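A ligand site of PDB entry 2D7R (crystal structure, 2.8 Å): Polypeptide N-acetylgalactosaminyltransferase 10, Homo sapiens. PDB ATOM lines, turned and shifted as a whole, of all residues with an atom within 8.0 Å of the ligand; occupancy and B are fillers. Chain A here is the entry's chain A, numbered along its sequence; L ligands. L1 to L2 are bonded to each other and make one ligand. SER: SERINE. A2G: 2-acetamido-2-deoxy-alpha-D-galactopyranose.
The backbone carbonyl oxygen (O) of Asn 511 sits at hydrogen-bond distance from the backbone NH (N) of Ala 493. A ring nitrogen (NE2) of His 524 lies within hydrogen-bond range of the backbone carbonyl oxygen (O) of Asn 511 (3.3 Å). O of Thr 501 lies within hydrogen-bond range of N of Asp 492 (2.7 Å). A ring nitrogen (NE2) of His 506 sits at hydrogen-bond distance from the side-chain amide oxygen (OE1) of Gln 512 (3.3 Å). The backbone carbonyl oxygen (O) of Met 508 lies close to a ring nitrogen (ND1) of His 506 (3.4 Å). The backbone NH (N) of Cys 490 sits at hydrogen-bond distance from the backbone carbonyl oxygen (O) of Tyr 503 (3.0 Å). The backbone carbonyl oxygen (O) of Gly 510 lies within hydrogen-bond range of a ring nitrogen (NE2) of His 524 (3.3 Å). The side-chain sulfur (SG) of Cys 505 forms a disulfide with the side-chain sulfur (SG) of Cys 490, at 2.0 Å.
The backbone NH (N) of Asn 511 is in hydrogen-bond range of an oxygen (O7) of A2G L2, at 2.7 Å. O4 of A2G L2 lies within hydrogen-bond range of ND2 of Asn 511 (2.6 Å). OD2 of Asp 492 sits at hydrogen-bond distance from O4 of A2G L2, 2.7 Å away. NE2 of His 506 sits at hydrogen-bond distance from O3 of A2G L2.
Residues that only touch the ligand: Tyr 503 and Gly 510. Hydrophobic or aromatic side chains that line the ligand: Tyr 503 and His 506. Along chain A the residues within 4 Å of the ligand span positions 492 to 511.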
ATOM      1  N   ALA A 247     -29.951  36.280  -8.509  1.00  0.00           N
ATOM      2  CA  ALA A 247     -29.391  36.434  -7.181  1.00  0.00           C
ATOM      3  C   ALA A 247     -28.890  37.877  -6.918  1.00  0.00           C
ATOM      4  O   ALA A 247     -28.195  38.476  -7.750  1.00  0.00           O
ATOM      5  CB  ALA A 247     -28.251  35.449  -7.005  1.00  0.00           C
ATOM      6  N   GLY A 248     -29.258  38.426  -5.772  1.00  0.00           N
ATOM      7  CA  GLY A 248     -28.815  39.751  -5.427  1.00  0.00           C
ATOM      8  C   GLY A 248     -29.472  40.855  -6.199  1.00  0.00           C
ATOM      9  O   GLY A 248     -29.153  42.028  -5.991  1.00  0.00           O
ATOM     10  N   CYS A 490     -15.209  26.533  -2.891  1.00  0.00           N
ATOM     11  CA  CYS A 490     -14.753  27.001  -1.585  1.00  0.00           C
ATOM     12  C   CYS A 490     -15.275  26.153  -0.433  1.00  0.00           C
ATOM     13  O   CYS A 490     -16.204  25.367  -0.613  1.00  0.00           O
ATOM     14  CB  CYS A 490     -15.182  28.472  -1.403  1.00  0.00           C
ATOM     15  SG  CYS A 490     -14.117  29.649  -2.308  1.00  0.00           S
ATOM     16  N   PHE A 491     -14.670  26.304   0.744  1.00  0.00           N
ATOM     17  CA  PHE A 491     -15.107  25.555   1.913  1.00  0.00           C
ATOM     18  C   PHE A 491     -16.419  26.139   2.447  1.00  0.00           C
ATOM     19  O   PHE A 491     -16.408  27.110   3.207  1.00  0.00           O
ATOM     20  CB  PHE A 491     -14.033  25.582   3.005  1.00  0.00           C
ATOM     21  CG  PHE A 491     -12.956  24.542   2.849  1.00  0.00           C
ATOM     22  CD1 PHE A 491     -12.043  24.304   3.879  1.00  0.00           C
ATOM     23  CD2 PHE A 491     -12.850  23.779   1.687  1.00  0.00           C
ATOM     24  CE1 PHE A 491     -11.049  23.347   3.750  1.00  0.00           C
ATOM     25  CE2 PHE A 491     -11.859  22.808   1.550  1.00  0.00           C
ATOM     26  CZ  PHE A 491     -10.956  22.600   2.590  1.00  0.00           C
ATOM     27  N   ASP A 492     -17.537  25.514   2.066  1.00  0.00           N
ATOM     28  CA  ASP A 492     -18.878  25.976   2.453  1.00  0.00           C
ATOM     29  C   ASP A 492     -19.444  25.214   3.661  1.00  0.00           C
ATOM     30  O   ASP A 492     -19.630  23.989   3.596  1.00  0.00           O
ATOM     31  CB  ASP A 492     -19.816  25.819   1.249  1.00  0.00           C
ATOM     32  CG  ASP A 492     -20.966  26.818   1.263  1.00  0.00           C
ATOM     33  OD1 ASP A 492     -20.682  28.029   1.363  1.00  0.00           O
ATOM     34  OD2 ASP A 492     -22.130  26.388   1.160  1.00  0.00           O
ATOM     35  N   ALA A 493     -19.718  25.937   4.741  1.00  0.00           N
ATOM     36  CA  ALA A 493     -20.254  25.333   5.967  1.00  0.00           C
ATOM     37  C   ALA A 493     -21.402  26.135   6.534  1.00  0.00           C
ATOM     38  O   ALA A 493     -21.251  27.308   6.898  1.00  0.00           O
ATOM     39  CB  ALA A 493     -19.147  25.210   7.001  1.00  0.00           C
ATOM     40  N   ILE A 494     -22.574  25.503   6.653  1.00  0.00           N
ATOM     41  CA  ILE A 494     -23.760  26.173   7.172  1.00  0.00           C
ATOM     42  C   ILE A 494     -23.790  26.125   8.695  1.00  0.00           C
ATOM     43  O   ILE A 494     -23.122  26.910   9.372  1.00  0.00           O
ATOM     44  CB  ILE A 494     -25.050  25.530   6.635  1.00  0.00           C
ATOM     45  CG1 ILE A 494     -24.966  25.356   5.117  1.00  0.00           C
ATOM     46  CG2 ILE A 494     -26.254  26.416   6.970  1.00  0.00           C
ATOM     47  CD1 ILE A 494     -26.115  24.580   4.510  1.00  0.00           C
ATOM     48  N   THR A 501     -18.590  21.373   2.873  1.00  0.00           N
ATOM     49  CA  THR A 501     -18.641  20.995   1.469  1.00  0.00           C
ATOM     50  C   THR A 501     -17.925  21.985   0.570  1.00  0.00           C
ATOM     51  O   THR A 501     -17.376  22.984   1.020  1.00  0.00           O
ATOM     52  CB  THR A 501     -20.096  20.849   0.942  1.00  0.00           C
ATOM     53  OG1 THR A 501     -20.829  22.045   1.253  1.00  0.00           O
ATOM     54  CG2 THR A 501     -20.761  19.641   1.554  1.00  0.00           C
ATOM     55  N   LEU A 502     -17.917  21.667  -0.722  1.00  0.00           N
ATOM     56  CA  LEU A 502     -17.300  22.506  -1.723  1.00  0.00           C
ATOM     57  C   LEU A 502     -18.386  23.093  -2.609  1.00  0.00           C
ATOM     58  O   LEU A 502     -18.806  22.481  -3.587  1.00  0.00           O
ATOM     59  CB  LEU A 502     -16.324  21.693  -2.573  1.00  0.00           C
ATOM     60  CG  LEU A 502     -15.077  21.131  -1.873  1.00  0.00           C
ATOM     61  CD1 LEU A 502     -14.291  20.280  -2.862  1.00  0.00           C
ATOM     62  CD2 LEU A 502     -14.218  22.270  -1.351  1.00  0.00           C
ATOM     63  N   TYR A 503     -18.852  24.286  -2.242  1.00  0.00           N
ATOM     64  CA  TYR A 503     -19.878  24.960  -3.019  1.00  0.00           C
ATOM     65  C   TYR A 503     -19.207  26.060  -3.842  1.00  0.00           C
ATOM     66  O   TYR A 503     -18.111  26.510  -3.500  1.00  0.00           O
ATOM     67  CB  TYR A 503     -20.941  25.565  -2.091  1.00  0.00           C
ATOM     68  CG  TYR A 503     -22.241  25.865  -2.791  1.00  0.00           C
ATOM     69  CD1 TYR A 503     -22.928  24.861  -3.461  1.00  0.00           C
ATOM     70  CD2 TYR A 503     -22.756  27.159  -2.817  1.00  0.00           C
ATOM     71  CE1 TYR A 503     -24.107  25.131  -4.142  1.00  0.00           C
ATOM     72  CE2 TYR A 503     -23.944  27.436  -3.507  1.00  0.00           C
ATOM     73  CZ  TYR A 503     -24.616  26.418  -4.170  1.00  0.00           C
ATOM     74  OH  TYR A 503     -25.781  26.673  -4.854  1.00  0.00           O
ATOM     75  N   ASP A 504     -19.838  26.474  -4.931  1.00  0.00           N
ATOM     76  CA  ASP A 504     -19.268  27.526  -5.760  1.00  0.00           C
ATOM     77  C   ASP A 504     -18.875  28.706  -4.873  1.00  0.00           C
ATOM     78  O   ASP A 504     -19.612  29.076  -3.966  1.00  0.00           O
ATOM     79  CB  ASP A 504     -20.293  27.974  -6.788  1.00  0.00           C
ATOM     80  CG  ASP A 504     -20.890  26.823  -7.545  1.00  0.00           C
ATOM     81  OD1 ASP A 504     -20.136  26.125  -8.246  1.00  0.00           O
ATOM     82  OD2 ASP A 504     -22.120  26.610  -7.439  1.00  0.00           O
ATOM     83  N   CYS A 505     -17.709  29.279  -5.151  1.00  0.00           N
ATOM     84  CA  CYS A 505     -17.241  30.408  -4.375  1.00  0.00           C
ATOM     85  C   CYS A 505     -18.038  31.656  -4.722  1.00  0.00           C
ATOM     86  O   CYS A 505     -19.026  31.602  -5.438  1.00  0.00           O
ATOM     87  CB  CYS A 505     -15.769  30.687  -4.653  1.00  0.00           C
ATOM     88  SG  CYS A 505     -14.569  29.373  -4.274  1.00  0.00           S
ATOM     89  N   HIS A 506     -17.556  32.785  -4.201  1.00  0.00           N
ATOM     90  CA  HIS A 506     -18.155  34.091  -4.413  1.00  0.00           C
ATOM     91  C   HIS A 506     -17.496  34.985  -3.388  1.00  0.00           C
ATOM     92  O   HIS A 506     -17.438  34.655  -2.209  1.00  0.00           O
ATOM     93  CB  HIS A 506     -19.672  34.068  -4.220  1.00  0.00           C
ATOM     94  CG  HIS A 506     -20.105  33.461  -2.920  1.00  0.00           C
ATOM     95  ND1 HIS A 506     -19.836  34.033  -1.694  1.00  0.00           N
ATOM     96  CD2 HIS A 506     -20.801  32.323  -2.652  1.00  0.00           C
ATOM     97  CE1 HIS A 506     -20.335  33.277  -0.737  1.00  0.00           C
ATOM     98  NE2 HIS A 506     -20.926  32.232  -1.296  1.00  0.00           N
ATOM     99  N   MET A 508     -17.963  36.928  -1.218  1.00  0.00           N
ATOM    100  CA  MET A 508     -18.921  37.428  -0.237  1.00  0.00           C
ATOM    101  C   MET A 508     -18.695  36.650   1.062  1.00  0.00           C
ATOM    102  O   MET A 508     -19.336  35.630   1.312  1.00  0.00           O
ATOM    103  CB  MET A 508     -20.346  37.184  -0.741  1.00  0.00           C
ATOM    104  CG  MET A 508     -20.545  37.469  -2.241  1.00  0.00           C
ATOM    105  SD  MET A 508     -20.473  39.207  -2.727  1.00  0.00           S
ATOM    106  CE  MET A 508     -22.245  39.610  -2.815  1.00  0.00           C
ATOM    107  N   LYS A 509     -17.774  37.150   1.880  1.00  0.00           N
ATOM    108  CA  LYS A 509     -17.419  36.530   3.156  1.00  0.00           C
ATOM    109  C   LYS A 509     -18.609  36.107   4.025  1.00  0.00           C
ATOM    110  O   LYS A 509     -19.032  36.836   4.918  1.00  0.00           O
ATOM    111  CB  LYS A 509     -16.512  37.477   3.955  1.00  0.00           C
ATOM    112  CG  LYS A 509     -15.371  38.026   3.120  1.00  0.00           C
ATOM    113  CD  LYS A 509     -14.448  38.922   3.910  1.00  0.00           C
ATOM    114  CE  LYS A 509     -13.507  39.673   2.978  1.00  0.00           C
ATOM    115  NZ  LYS A 509     -12.772  38.767   2.051  1.00  0.00           N
ATOM    116  N   GLY A 510     -19.129  34.919   3.741  1.00  0.00           N
ATOM    117  CA  GLY A 510     -20.252  34.411   4.504  1.00  0.00           C
ATOM    118  C   GLY A 510     -19.997  32.988   4.977  1.00  0.00           C
ATOM    119  O   GLY A 510     -19.313  32.755   5.981  1.00  0.00           O
ATOM    120  N   ASN A 511     -20.564  32.032   4.256  1.00  0.00           N
ATOM    121  CA  ASN A 511     -20.401  30.632   4.586  1.00  0.00           C
ATOM    122  C   ASN A 511     -19.037  30.156   4.079  1.00  0.00           C
ATOM    123  O   ASN A 511     -18.652  29.009   4.308  1.00  0.00           O
ATOM    124  CB  ASN A 511     -21.509  29.806   3.929  1.00  0.00           C
ATOM    125  CG  ASN A 511     -22.855  30.080   4.545  1.00  0.00           C
ATOM    126  OD1 ASN A 511     -23.035  31.084   5.223  1.00  0.00           O
ATOM    127  ND2 ASN A 511     -23.805  29.175   4.320  1.00  0.00           N
ATOM    128  N   GLN A 512     -18.310  31.041   3.397  1.00  0.00           N
ATOM    129  CA  GLN A 512     -16.999  30.712   2.850  1.00  0.00           C
ATOM    130  C   GLN A 512     -15.931  31.605   3.460  1.00  0.00           C
ATOM    131  O   GLN A 512     -14.857  31.795   2.900  1.00  0.00           O
ATOM    132  CB  GLN A 512     -17.026  30.883   1.332  1.00  0.00           C
ATOM    133  CG  GLN A 512     -18.057  30.024   0.644  1.00  0.00           C
ATOM    134  CD  GLN A 512     -18.078  30.211  -0.856  1.00  0.00           C
ATOM    135  OE1 GLN A 512     -18.887  29.613  -1.552  1.00  0.00           O
ATOM    136  NE2 GLN A 512     -17.181  31.053  -1.354  1.00  0.00           N
ATOM    137  N   LEU A 513     -16.240  32.147   4.631  1.00  0.00           N
ATOM    138  CA  LEU A 513     -15.318  33.014   5.350  1.00  0.00           C
ATOM    139  C   LEU A 513     -14.600  32.220   6.440  1.00  0.00           C
ATOM    140  O   LEU A 513     -15.237  31.698   7.353  1.00  0.00           O
ATOM    141  CB  LEU A 513     -16.086  34.181   5.977  1.00  0.00           C
ATOM    142  CG  LEU A 513     -15.434  35.014   7.095  1.00  0.00           C
ATOM    143  CD1 LEU A 513     -14.060  35.510   6.688  1.00  0.00           C
ATOM    144  CD2 LEU A 513     -16.355  36.194   7.400  1.00  0.00           C
ATOM    145  N   HIS A 524     -14.864  29.694  12.020  1.00  0.00           N
ATOM    146  CA  HIS A 524     -15.881  30.108  11.077  1.00  0.00           C
ATOM    147  C   HIS A 524     -16.807  31.078  11.813  1.00  0.00           C
ATOM    148  O   HIS A 524     -17.751  30.652  12.462  1.00  0.00           O
ATOM    149  CB  HIS A 524     -16.694  28.908  10.600  1.00  0.00           C
ATOM    150  CG  HIS A 524     -17.502  29.178   9.368  1.00  0.00           C
ATOM    151  ND1 HIS A 524     -18.468  28.312   8.903  1.00  0.00           N
ATOM    152  CD2 HIS A 524     -17.461  30.205   8.478  1.00  0.00           C
ATOM    153  CE1 HIS A 524     -18.980  28.783   7.783  1.00  0.00           C
ATOM    154  NE2 HIS A 524     -18.390  29.937   7.503  1.00  0.00           N
ATOM    155  N   VAL A 526     -19.190  33.131  10.813  1.00  0.00           N
ATOM    156  CA  VAL A 526     -20.594  33.132  10.404  1.00  0.00           C
ATOM    157  C   VAL A 526     -21.366  31.964  11.022  1.00  0.00           C
ATOM    158  O   VAL A 526     -22.593  31.898  10.902  1.00  0.00           O
ATOM    159  CB  VAL A 526     -20.720  33.047   8.856  1.00  0.00           C
ATOM    160  CG1 VAL A 526     -20.605  31.613   8.398  1.00  0.00           C
ATOM    161  CG2 VAL A 526     -22.036  33.653   8.414  1.00  0.00           C
HETATM  162  N   SER L   1     -27.897  32.838  -2.094  1.00  0.00           N
HETATM  163  CA  SER L   1     -27.921  33.297  -0.686  1.00  0.00           C
HETATM  164  C   SER L   1     -26.771  34.293  -0.352  1.00  0.00           C
HETATM  165  O   SER L   1     -26.971  35.274   0.366  1.00  0.00           O
HETATM  166  CB  SER L   1     -27.883  32.066   0.242  1.00  0.00           C
HETATM  167  OG  SER L   1     -26.625  31.371   0.176  1.00  0.00           O
HETATM  168  OXT SER L   1     -25.636  34.102  -0.797  1.00  0.00           O
HETATM  169  O5  A2G L   2     -26.215  29.375   1.383  1.00  0.00           O
HETATM  170  C1  A2G L   2     -26.070  30.829   1.385  1.00  0.00           C
HETATM  171  C2  A2G L   2     -24.571  31.238   1.526  1.00  0.00           C
HETATM  172  N2  A2G L   2     -24.488  32.684   1.495  1.00  0.00           N
HETATM  173  C3  A2G L   2     -23.753  30.571   0.404  1.00  0.00           C
HETATM  174  O3  A2G L   2     -22.375  30.917   0.525  1.00  0.00           O
HETATM  175  C4  A2G L   2     -23.914  29.048   0.487  1.00  0.00           C
HETATM  176  O4  A2G L   2     -23.424  28.624   1.777  1.00  0.00           O
HETATM  177  C5  A2G L   2     -25.405  28.712   0.357  1.00  0.00           C
HETATM  178  C6  A2G L   2     -25.603  27.211   0.439  1.00  0.00           C
HETATM  179  O6  A2G L   2     -25.211  26.677  -0.831  1.00  0.00           O
HETATM  180  C7  A2G L   2     -23.584  33.387   2.214  1.00  0.00           C
HETATM  181  O7  A2G L   2     -22.779  32.835   2.940  1.00  0.00           O
HETATM  182  C8  A2G L   2     -23.646  34.888   2.053  1.00  0.00           C
